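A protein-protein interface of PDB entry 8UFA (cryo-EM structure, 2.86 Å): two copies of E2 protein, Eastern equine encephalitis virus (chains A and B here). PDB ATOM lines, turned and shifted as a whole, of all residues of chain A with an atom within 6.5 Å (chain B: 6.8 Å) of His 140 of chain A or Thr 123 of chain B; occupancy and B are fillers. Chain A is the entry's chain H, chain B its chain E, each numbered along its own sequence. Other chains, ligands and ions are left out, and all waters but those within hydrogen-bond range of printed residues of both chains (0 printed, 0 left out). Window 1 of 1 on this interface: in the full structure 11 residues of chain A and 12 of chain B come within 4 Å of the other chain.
Among the printed residues, merely in contact across the chains: His 140 of chain A with Asn 21 of chain B (3.4 Å), His 140 of chain A with Thr 108 of chain B (3.3 Å), His 140 of chain A with Thr 123 of chain B (3.9 Å), His 140 of chain A with Ala 125 of chain B (3.8 Å), Glu 143 of chain A with Pro 20 of chain B (3.5 Å) and Glu 143 of chain A with Val 124 of chain B (3.8 Å).
No position is printed for both chains.
Of the 9 pairs that touch across the chains among the printed residues, none has its exchanged pair printed and touching as well.
OG of Ser 90 of chain A sits at hydrogen-bond distance from O of Gly 23 of chain B (3.3 Å).
The guanidinium group (NH1) of Arg 139 of chain A is in salt-bridge range of the side-chain carboxylate (OD1) of Asp 107 of chain B, 3.1 Å away.
OE2 of Glu 143 of chain A is in hydrogen-bond range of N of Ala 125 of chain B.
Of the 11 printed residues of chain A, 4 touch a printed residue of chain B.
Along chain A the printed residues that touch a printed residue of chain B span positions 90 to 143.
Hydrophobic or aromatic side chains of chain B within 4 Å of the printed part of chain A: Pro 20, Val 124 and Ala 125.
Among the printed residues, Asp or Glu carboxylates within 4 Å of a Lys or Arg side-chain nitrogen of the other chain: Arg 139 of chain A with Asp 107 of chain B.
The backbone carbonyl oxygen (O) of Thr 123 of chain B is in hydrogen-bond range of the side-chain amide nitrogen (ND2) of Asn 21 of chain B.
The backbone carbonyl oxygen of His 126 of chain B is in hydrogen-bond range of the backbone NH of Thr 108 of chain B (3.4 Å).
OG1 of Thr 110 of chain B is in hydrogen-bond range of OG1 of Thr 123 of chain B (2.9 Å).
O of Asp 107 of chain B is in hydrogen-bond range of N of His 126 of chain B, 3.0 Å away.
SG of Cys 19 of chain B lies close to N of Asn 21 of chain B (3.5 Å).
The side-chain sulfur (SG) of Cys 19 of chain B is disulfide-bonded to the side-chain sulfur (SG) of Cys 122 of chain B.
Of chain B, only Asn 21, Thr 108, Thr 123 and Ala 125 come within 4 Å of His 140 of chain A.
Thr 123 of chain B touches one residue of chain A.
Of the printed residues of chain B, Arg 139 of chain A touches Asp 107 (3.1 Å).
Of the printed residues of chain A, Gly 23 of chain B touches Ser 90.
Printed residues of chain A within 4 Å of Ala 125 of chain B: His 140 and Glu 143.
Val 109 of chain B touches none of the printed residues of chain A.
Pro 141 of chain A touches none of the printed residues of chain B.
The nearest residue of chain B that does not touch His 140 of chain A is Val 124 of chain B (4.4 Å).
The nearest residue of chain A that does not touch Thr 123 of chain B is Glu 143 of chain A (5.5 Å).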
ATOM      1  N   SER A  90     -13.024  -4.126 -29.468  1.00  0.00           N
ATOM      2  CA  SER A  90     -13.229  -5.455 -28.915  1.00  0.00           C
ATOM      3  C   SER A  90     -14.324  -5.386 -27.861  1.00  0.00           C
ATOM      4  O   SER A  90     -14.296  -4.516 -26.987  1.00  0.00           O
ATOM      5  CB  SER A  90     -11.934  -5.991 -28.305  1.00  0.00           C
ATOM      6  OG  SER A  90     -10.917  -6.097 -29.284  1.00  0.00           O
ATOM      7  N   PHE A 130      -7.172   7.602 -25.436  1.00  0.00           N
ATOM      8  CA  PHE A 130      -6.384   6.585 -24.761  1.00  0.00           C
ATOM      9  C   PHE A 130      -5.625   7.279 -23.643  1.00  0.00           C
ATOM     10  O   PHE A 130      -4.996   8.318 -23.868  1.00  0.00           O
ATOM     11  CB  PHE A 130      -5.411   5.890 -25.712  1.00  0.00           C
ATOM     12  CG  PHE A 130      -4.700   4.726 -25.093  1.00  0.00           C
ATOM     13  CD1 PHE A 130      -5.330   3.505 -24.982  1.00  0.00           C
ATOM     14  CD2 PHE A 130      -3.403   4.846 -24.639  1.00  0.00           C
ATOM     15  CE1 PHE A 130      -4.686   2.432 -24.428  1.00  0.00           C
ATOM     16  CE2 PHE A 130      -2.752   3.772 -24.084  1.00  0.00           C
ATOM     17  CZ  PHE A 130      -3.397   2.564 -23.971  1.00  0.00           C
ATOM     18  N   TYR A 138       2.301   5.998 -23.878  1.00  0.00           N
ATOM     19  CA  TYR A 138       2.170   4.918 -24.843  1.00  0.00           C
ATOM     20  C   TYR A 138       0.778   4.947 -25.476  1.00  0.00           C
ATOM     21  O   TYR A 138      -0.184   5.462 -24.900  1.00  0.00           O
ATOM     22  CB  TYR A 138       2.456   3.564 -24.190  1.00  0.00           C
ATOM     23  CG  TYR A 138       1.599   3.227 -22.991  1.00  0.00           C
ATOM     24  CD1 TYR A 138       0.393   2.574 -23.140  1.00  0.00           C
ATOM     25  CD2 TYR A 138       2.017   3.538 -21.710  1.00  0.00           C
ATOM     26  CE1 TYR A 138      -0.379   2.248 -22.054  1.00  0.00           C
ATOM     27  CE2 TYR A 138       1.251   3.217 -20.615  1.00  0.00           C
ATOM     28  CZ  TYR A 138       0.051   2.574 -20.792  1.00  0.00           C
ATOM     29  OH  TYR A 138      -0.732   2.263 -19.707  1.00  0.00           O
ATOM     30  N   ARG A 139       0.678   4.383 -26.679  1.00  0.00           N
ATOM     31  CA  ARG A 139      -0.551   4.431 -27.461  1.00  0.00           C
ATOM     32  C   ARG A 139      -1.338   3.127 -27.457  1.00  0.00           C
ATOM     33  O   ARG A 139      -2.423   3.081 -28.042  1.00  0.00           O
ATOM     34  CB  ARG A 139      -0.231   4.815 -28.907  1.00  0.00           C
ATOM     35  CG  ARG A 139       0.387   6.191 -29.068  1.00  0.00           C
ATOM     36  CD  ARG A 139       0.649   6.497 -30.531  1.00  0.00           C
ATOM     37  NE  ARG A 139       1.208   7.827 -30.735  1.00  0.00           N
ATOM     38  CZ  ARG A 139       1.561   8.316 -31.916  1.00  0.00           C
ATOM     39  NH1 ARG A 139       1.437   7.604 -33.026  1.00  0.00           N
ATOM     40  NH2 ARG A 139       2.052   9.550 -31.987  1.00  0.00           N
ATOM     41  N   HIS A 140      -0.834   2.072 -26.815  1.00  0.00           N
ATOM     42  CA  HIS A 140      -1.572   0.821 -26.748  1.00  0.00           C
ATOM     43  C   HIS A 140      -0.986   0.010 -25.606  1.00  0.00           C
ATOM     44  O   HIS A 140       0.230   0.083 -25.385  1.00  0.00           O
ATOM     45  CB  HIS A 140      -1.495   0.056 -28.076  1.00  0.00           C
ATOM     46  CG  HIS A 140      -2.438  -1.103 -28.168  1.00  0.00           C
ATOM     47  ND1 HIS A 140      -2.031  -2.412 -28.022  1.00  0.00           N
ATOM     48  CD2 HIS A 140      -3.779  -1.146 -28.350  1.00  0.00           C
ATOM     49  CE1 HIS A 140      -3.079  -3.211 -28.123  1.00  0.00           C
ATOM     50  NE2 HIS A 140      -4.150  -2.468 -28.330  1.00  0.00           N
ATOM     51  N   PRO A 141      -1.789  -0.748 -24.861  1.00  0.00           N
ATOM     52  CA  PRO A 141      -1.259  -1.498 -23.716  1.00  0.00           C
ATOM     53  C   PRO A 141      -0.031  -2.310 -24.089  1.00  0.00           C
ATOM     54  O   PRO A 141      -0.047  -3.067 -25.072  1.00  0.00           O
ATOM     55  CB  PRO A 141      -2.434  -2.404 -23.323  1.00  0.00           C
ATOM     56  CG  PRO A 141      -3.621  -1.613 -23.704  1.00  0.00           C
ATOM     57  CD  PRO A 141      -3.246  -0.939 -24.989  1.00  0.00           C
ATOM     58  N   PRO A 142       1.059  -2.181 -23.333  1.00  0.00           N
ATOM     59  CA  PRO A 142       2.272  -2.933 -23.656  1.00  0.00           C
ATOM     60  C   PRO A 142       2.151  -4.411 -23.328  1.00  0.00           C
ATOM     61  O   PRO A 142       1.331  -4.845 -22.517  1.00  0.00           O
ATOM     62  CB  PRO A 142       3.347  -2.274 -22.783  1.00  0.00           C
ATOM     63  CG  PRO A 142       2.774  -0.994 -22.372  1.00  0.00           C
ATOM     64  CD  PRO A 142       1.320  -1.230 -22.243  1.00  0.00           C
ATOM     65  N   GLU A 143       2.996  -5.189 -24.001  1.00  0.00           N
ATOM     66  CA  GLU A 143       3.100  -6.610 -23.705  1.00  0.00           C
ATOM     67  C   GLU A 143       3.779  -6.829 -22.363  1.00  0.00           C
ATOM     68  O   GLU A 143       3.462  -7.789 -21.651  1.00  0.00           O
ATOM     69  CB  GLU A 143       3.889  -7.316 -24.809  1.00  0.00           C
ATOM     70  CG  GLU A 143       3.242  -7.233 -26.178  1.00  0.00           C
ATOM     71  CD  GLU A 143       3.450  -5.895 -26.867  1.00  0.00           C
ATOM     72  OE1 GLU A 143       4.281  -5.093 -26.389  1.00  0.00           O
ATOM     73  OE2 GLU A 143       2.770  -5.643 -27.883  1.00  0.00           O
ATOM     74  N   ILE A 264      -0.420  -2.530 -17.064  1.00  0.00           N
ATOM     75  CA  ILE A 264       0.979  -2.569 -17.470  1.00  0.00           C
ATOM     76  C   ILE A 264       1.304  -1.273 -18.199  1.00  0.00           C
ATOM     77  O   ILE A 264       0.600  -0.879 -19.135  1.00  0.00           O
ATOM     78  CB  ILE A 264       1.270  -3.792 -18.358  1.00  0.00           C
ATOM     79  CG1 ILE A 264       1.012  -5.090 -17.593  1.00  0.00           C
ATOM     80  CG2 ILE A 264       2.708  -3.767 -18.860  1.00  0.00           C
ATOM     81  CD1 ILE A 264       1.041  -6.318 -18.470  1.00  0.00           C
ATOM     82  N   THR A 266       4.612   1.079 -19.987  1.00  0.00           N
ATOM     83  CA  THR A 266       5.898   0.873 -20.630  1.00  0.00           C
ATOM     84  C   THR A 266       7.051   1.242 -19.701  1.00  0.00           C
ATOM     85  O   THR A 266       6.892   1.957 -18.709  1.00  0.00           O
ATOM     86  CB  THR A 266       6.002   1.707 -21.907  1.00  0.00           C
ATOM     87  OG1 THR A 266       5.722   3.078 -21.609  1.00  0.00           O
ATOM     88  CG2 THR A 266       5.031   1.221 -22.949  1.00  0.00           C
ATOM     89  N   HIS A 288       8.436   6.362 -26.562  1.00  0.00           N
ATOM     90  CA  HIS A 288       7.223   7.151 -26.474  1.00  0.00           C
ATOM     91  C   HIS A 288       7.572   8.408 -25.699  1.00  0.00           C
ATOM     92  O   HIS A 288       8.598   8.449 -25.013  1.00  0.00           O
ATOM     93  CB  HIS A 288       6.106   6.400 -25.738  1.00  0.00           C
ATOM     94  CG  HIS A 288       5.843   5.026 -26.267  1.00  0.00           C
ATOM     95  ND1 HIS A 288       5.200   4.794 -27.463  1.00  0.00           N
ATOM     96  CD2 HIS A 288       6.136   3.808 -25.755  1.00  0.00           C
ATOM     97  CE1 HIS A 288       5.115   3.492 -27.669  1.00  0.00           C
ATOM     98  NE2 HIS A 288       5.674   2.872 -26.646  1.00  0.00           N
ATOM     99  N   CYS B  19      -0.359 -14.397 -26.454  1.00  0.00           N
ATOM    100  CA  CYS B  19      -0.708 -13.211 -27.211  1.00  0.00           C
ATOM    101  C   CYS B  19      -1.152 -12.120 -26.246  1.00  0.00           C
ATOM    102  O   CYS B  19      -2.046 -12.358 -25.424  1.00  0.00           O
ATOM    103  CB  CYS B  19      -1.825 -13.490 -28.225  1.00  0.00           C
ATOM    104  SG  CYS B  19      -2.419 -11.985 -29.039  1.00  0.00           S
ATOM    105  N   PRO B  20      -0.566 -10.923 -26.307  1.00  0.00           N
ATOM    106  CA  PRO B  20      -0.947  -9.874 -25.351  1.00  0.00           C
ATOM    107  C   PRO B  20      -2.406  -9.459 -25.419  1.00  0.00           C
ATOM    108  O   PRO B  20      -2.938  -8.967 -24.416  1.00  0.00           O
ATOM    109  CB  PRO B  20      -0.015  -8.717 -25.726  1.00  0.00           C
ATOM    110  CG  PRO B  20       0.323  -8.960 -27.150  1.00  0.00           C
ATOM    111  CD  PRO B  20       0.429 -10.435 -27.275  1.00  0.00           C
ATOM    112  N   ASN B  21      -3.078  -9.635 -26.557  1.00  0.00           N
ATOM    113  CA  ASN B  21      -4.486  -9.257 -26.682  1.00  0.00           C
ATOM    114  C   ASN B  21      -5.207 -10.269 -27.565  1.00  0.00           C
ATOM    115  O   ASN B  21      -5.058 -10.253 -28.789  1.00  0.00           O
ATOM    116  CB  ASN B  21      -4.636  -7.853 -27.258  1.00  0.00           C
ATOM    117  CG  ASN B  21      -3.957  -6.796 -26.415  1.00  0.00           C
ATOM    118  OD1 ASN B  21      -4.508  -6.337 -25.415  1.00  0.00           O
ATOM    119  ND2 ASN B  21      -2.767  -6.378 -26.835  1.00  0.00           N
ATOM    120  N   CYS B  22      -5.988 -11.142 -26.935  1.00  0.00           N
ATOM    121  CA  CYS B  22      -6.880 -12.055 -27.644  1.00  0.00           C
ATOM    122  C   CYS B  22      -8.270 -11.442 -27.522  1.00  0.00           C
ATOM    123  O   CYS B  22      -9.068 -11.804 -26.659  1.00  0.00           O
ATOM    124  CB  CYS B  22      -6.839 -13.449 -27.043  1.00  0.00           C
ATOM    125  SG  CYS B  22      -5.254 -14.262 -27.065  1.00  0.00           S
ATOM    126  N   GLY B  23      -8.563 -10.508 -28.413  1.00  0.00           N
ATOM    127  CA  GLY B  23      -9.762  -9.723 -28.235  1.00  0.00           C
ATOM    128  C   GLY B  23      -9.537  -8.695 -27.147  1.00  0.00           C
ATOM    129  O   GLY B  23      -8.778  -7.741 -27.339  1.00  0.00           O
ATOM    130  N   ILE B  33       1.296 -13.440 -32.742  1.00  0.00           N
ATOM    131  CA  ILE B  33       2.222 -12.697 -33.591  1.00  0.00           C
ATOM    132  C   ILE B  33       3.609 -12.741 -32.964  1.00  0.00           C
ATOM    133  O   ILE B  33       3.795 -12.330 -31.814  1.00  0.00           O
ATOM    134  CB  ILE B  33       1.755 -11.247 -33.780  1.00  0.00           C
ATOM    135  CG1 ILE B  33       0.387 -11.212 -34.464  1.00  0.00           C
ATOM    136  CG2 ILE B  33       2.782 -10.449 -34.580  1.00  0.00           C
ATOM    137  CD1 ILE B  33      -0.271  -9.857 -34.438  1.00  0.00           C
ATOM    138  N   ARG B  84      -5.156  -5.943 -39.582  1.00  0.00           N
ATOM    139  CA  ARG B  84      -5.580  -4.572 -39.347  1.00  0.00           C
ATOM    140  C   ARG B  84      -4.546  -3.857 -38.491  1.00  0.00           C
ATOM    141  O   ARG B  84      -4.010  -4.442 -37.548  1.00  0.00           O
ATOM    142  CB  ARG B  84      -6.949  -4.550 -38.653  1.00  0.00           C
ATOM    143  CG  ARG B  84      -7.472  -3.163 -38.336  1.00  0.00           C
ATOM    144  CD  ARG B  84      -8.889  -3.192 -37.777  1.00  0.00           C
ATOM    145  NE  ARG B  84      -8.943  -3.644 -36.389  1.00  0.00           N
ATOM    146  CZ  ARG B  84      -9.436  -4.804 -35.975  1.00  0.00           C
ATOM    147  NH1 ARG B  84      -9.887  -5.713 -36.826  1.00  0.00           N
ATOM    148  NH2 ARG B  84      -9.484  -5.058 -34.671  1.00  0.00           N
ATOM    149  N   ASP B 107      -0.910   2.235 -34.675  1.00  0.00           N
ATOM    150  CA  ASP B 107      -0.215   1.983 -33.421  1.00  0.00           C
ATOM    151  C   ASP B 107      -0.237   0.516 -33.021  1.00  0.00           C
ATOM    152  O   ASP B 107       0.457   0.138 -32.072  1.00  0.00           O
ATOM    153  CB  ASP B 107      -0.840   2.816 -32.292  1.00  0.00           C
ATOM    154  CG  ASP B 107      -0.769   4.305 -32.555  1.00  0.00           C
ATOM    155  OD1 ASP B 107       0.267   4.765 -33.075  1.00  0.00           O
ATOM    156  OD2 ASP B 107      -1.749   5.015 -32.245  1.00  0.00           O
ATOM    157  N   THR B 108      -1.015  -0.311 -33.714  1.00  0.00           N
ATOM    158  CA  THR B 108      -1.142  -1.725 -33.402  1.00  0.00           C
ATOM    159  C   THR B 108      -1.133  -2.519 -34.698  1.00  0.00           C
ATOM    160  O   THR B 108      -1.256  -1.965 -35.792  1.00  0.00           O
ATOM    161  CB  THR B 108      -2.432  -2.025 -32.631  1.00  0.00           C
ATOM    162  OG1 THR B 108      -3.558  -1.882 -33.505  1.00  0.00           O
ATOM    163  CG2 THR B 108      -2.592  -1.076 -31.469  1.00  0.00           C
ATOM    164  N   VAL B 109      -0.961  -3.828 -34.564  1.00  0.00           N
ATOM    165  CA  VAL B 109      -1.094  -4.766 -35.671  1.00  0.00           C
ATOM    166  C   VAL B 109      -1.998  -5.889 -35.190  1.00  0.00           C
ATOM    167  O   VAL B 109      -1.698  -6.545 -34.186  1.00  0.00           O
ATOM    168  CB  VAL B 109       0.264  -5.314 -36.141  1.00  0.00           C
ATOM    169  CG1 VAL B 109       0.075  -6.325 -37.257  1.00  0.00           C
ATOM    170  CG2 VAL B 109       1.153  -4.177 -36.614  1.00  0.00           C
ATOM    171  N   THR B 110      -3.100  -6.106 -35.897  1.00  0.00           N
ATOM    172  CA  THR B 110      -4.073  -7.131 -35.551  1.00  0.00           C
ATOM    173  C   THR B 110      -4.138  -8.163 -36.664  1.00  0.00           C
ATOM    174  O   THR B 110      -4.253  -7.806 -37.839  1.00  0.00           O
ATOM    175  CB  THR B 110      -5.457  -6.518 -35.327  1.00  0.00           C
ATOM    176  OG1 THR B 110      -5.379  -5.513 -34.310  1.00  0.00           O
ATOM    177  CG2 THR B 110      -6.443  -7.586 -34.896  1.00  0.00           C
ATOM    178  N   VAL B 111      -4.055  -9.434 -36.292  1.00  0.00           N
ATOM    179  CA  VAL B 111      -4.172 -10.546 -37.225  1.00  0.00           C
ATOM    180  C   VAL B 111      -5.187 -11.522 -36.650  1.00  0.00           C
ATOM    181  O   VAL B 111      -5.231 -11.733 -35.433  1.00  0.00           O
ATOM    182  CB  VAL B 111      -2.812 -11.236 -37.461  1.00  0.00           C
ATOM    183  CG1 VAL B 111      -2.944 -12.356 -38.476  1.00  0.00           C
ATOM    184  CG2 VAL B 111      -1.781 -10.218 -37.913  1.00  0.00           C
ATOM    185  N   THR B 121      -8.171 -13.925 -32.961  1.00  0.00           N
ATOM    186  CA  THR B 121      -7.415 -12.724 -33.290  1.00  0.00           C
ATOM    187  C   THR B 121      -6.282 -12.532 -32.289  1.00  0.00           C
ATOM    188  O   THR B 121      -6.306 -13.069 -31.181  1.00  0.00           O
ATOM    189  CB  THR B 121      -8.308 -11.473 -33.308  1.00  0.00           C
ATOM    190  OG1 THR B 121      -8.771 -11.189 -31.982  1.00  0.00           O
ATOM    191  CG2 THR B 121      -9.500 -11.679 -34.224  1.00  0.00           C
ATOM    192  N   CYS B 122      -5.277 -11.763 -32.705  1.00  0.00           N
ATOM    193  CA  CYS B 122      -4.159 -11.394 -31.844  1.00  0.00           C
ATOM    194  C   CYS B 122      -3.725  -9.983 -32.209  1.00  0.00           C
ATOM    195  O   CYS B 122      -3.390  -9.720 -33.367  1.00  0.00           O
ATOM    196  CB  CYS B 122      -2.989 -12.376 -31.982  1.00  0.00           C
ATOM    197  SG  CYS B 122      -1.592 -11.992 -30.895  1.00  0.00           S
ATOM    198  N   THR B 123      -3.740  -9.077 -31.232  1.00  0.00           N
ATOM    199  CA  THR B 123      -3.335  -7.689 -31.424  1.00  0.00           C
ATOM    200  C   THR B 123      -2.102  -7.390 -30.586  1.00  0.00           C
ATOM    201  O   THR B 123      -2.065  -7.709 -29.393  1.00  0.00           O
ATOM    202  CB  THR B 123      -4.460  -6.722 -31.042  1.00  0.00           C
ATOM    203  OG1 THR B 123      -5.638  -7.023 -31.800  1.00  0.00           O
ATOM    204  CG2 THR B 123      -4.043  -5.284 -31.310  1.00  0.00           C
ATOM    205  N   VAL B 124      -1.100  -6.780 -31.212  1.00  0.00           N
ATOM    206  CA  VAL B 124       0.132  -6.380 -30.544  1.00  0.00           C
ATOM    207  C   VAL B 124       0.346  -4.892 -30.778  1.00  0.00           C
ATOM    208  O   VAL B 124      -0.142  -4.322 -31.758  1.00  0.00           O
ATOM    209  CB  VAL B 124       1.353  -7.188 -31.039  1.00  0.00           C
ATOM    210  CG1 VAL B 124       1.135  -8.672 -30.811  1.00  0.00           C
ATOM    211  CG2 VAL B 124       1.636  -6.899 -32.505  1.00  0.00           C
ATOM    212  N   ALA B 125       1.077  -4.262 -29.864  1.00  0.00           N
ATOM    213  CA  ALA B 125       1.427  -2.856 -30.014  1.00  0.00           C
ATOM    214  C   ALA B 125       2.662  -2.752 -30.899  1.00  0.00           C
ATOM    215  O   ALA B 125       3.712  -3.320 -30.582  1.00  0.00           O
ATOM    216  CB  ALA B 125       1.682  -2.218 -28.651  1.00  0.00           C
ATOM    217  N   HIS B 126       2.537  -2.025 -32.004  1.00  0.00           N
ATOM    218  CA  HIS B 126       3.632  -1.883 -32.960  1.00  0.00           C
ATOM    219  C   HIS B 126       3.348  -0.673 -33.829  1.00  0.00           C
ATOM    220  O   HIS B 126       2.295  -0.609 -34.469  1.00  0.00           O
ATOM    221  CB  HIS B 126       3.777  -3.138 -33.822  1.00  0.00           C
ATOM    222  CG  HIS B 126       4.967  -3.111 -34.730  1.00  0.00           C
ATOM    223  ND1 HIS B 126       6.249  -3.358 -34.289  1.00  0.00           N
ATOM    224  CD2 HIS B 126       5.066  -2.880 -36.061  1.00  0.00           C
ATOM    225  CE1 HIS B 126       7.087  -3.267 -35.306  1.00  0.00           C
ATOM    226  NE2 HIS B 126       6.396  -2.979 -36.393  1.00  0.00           N
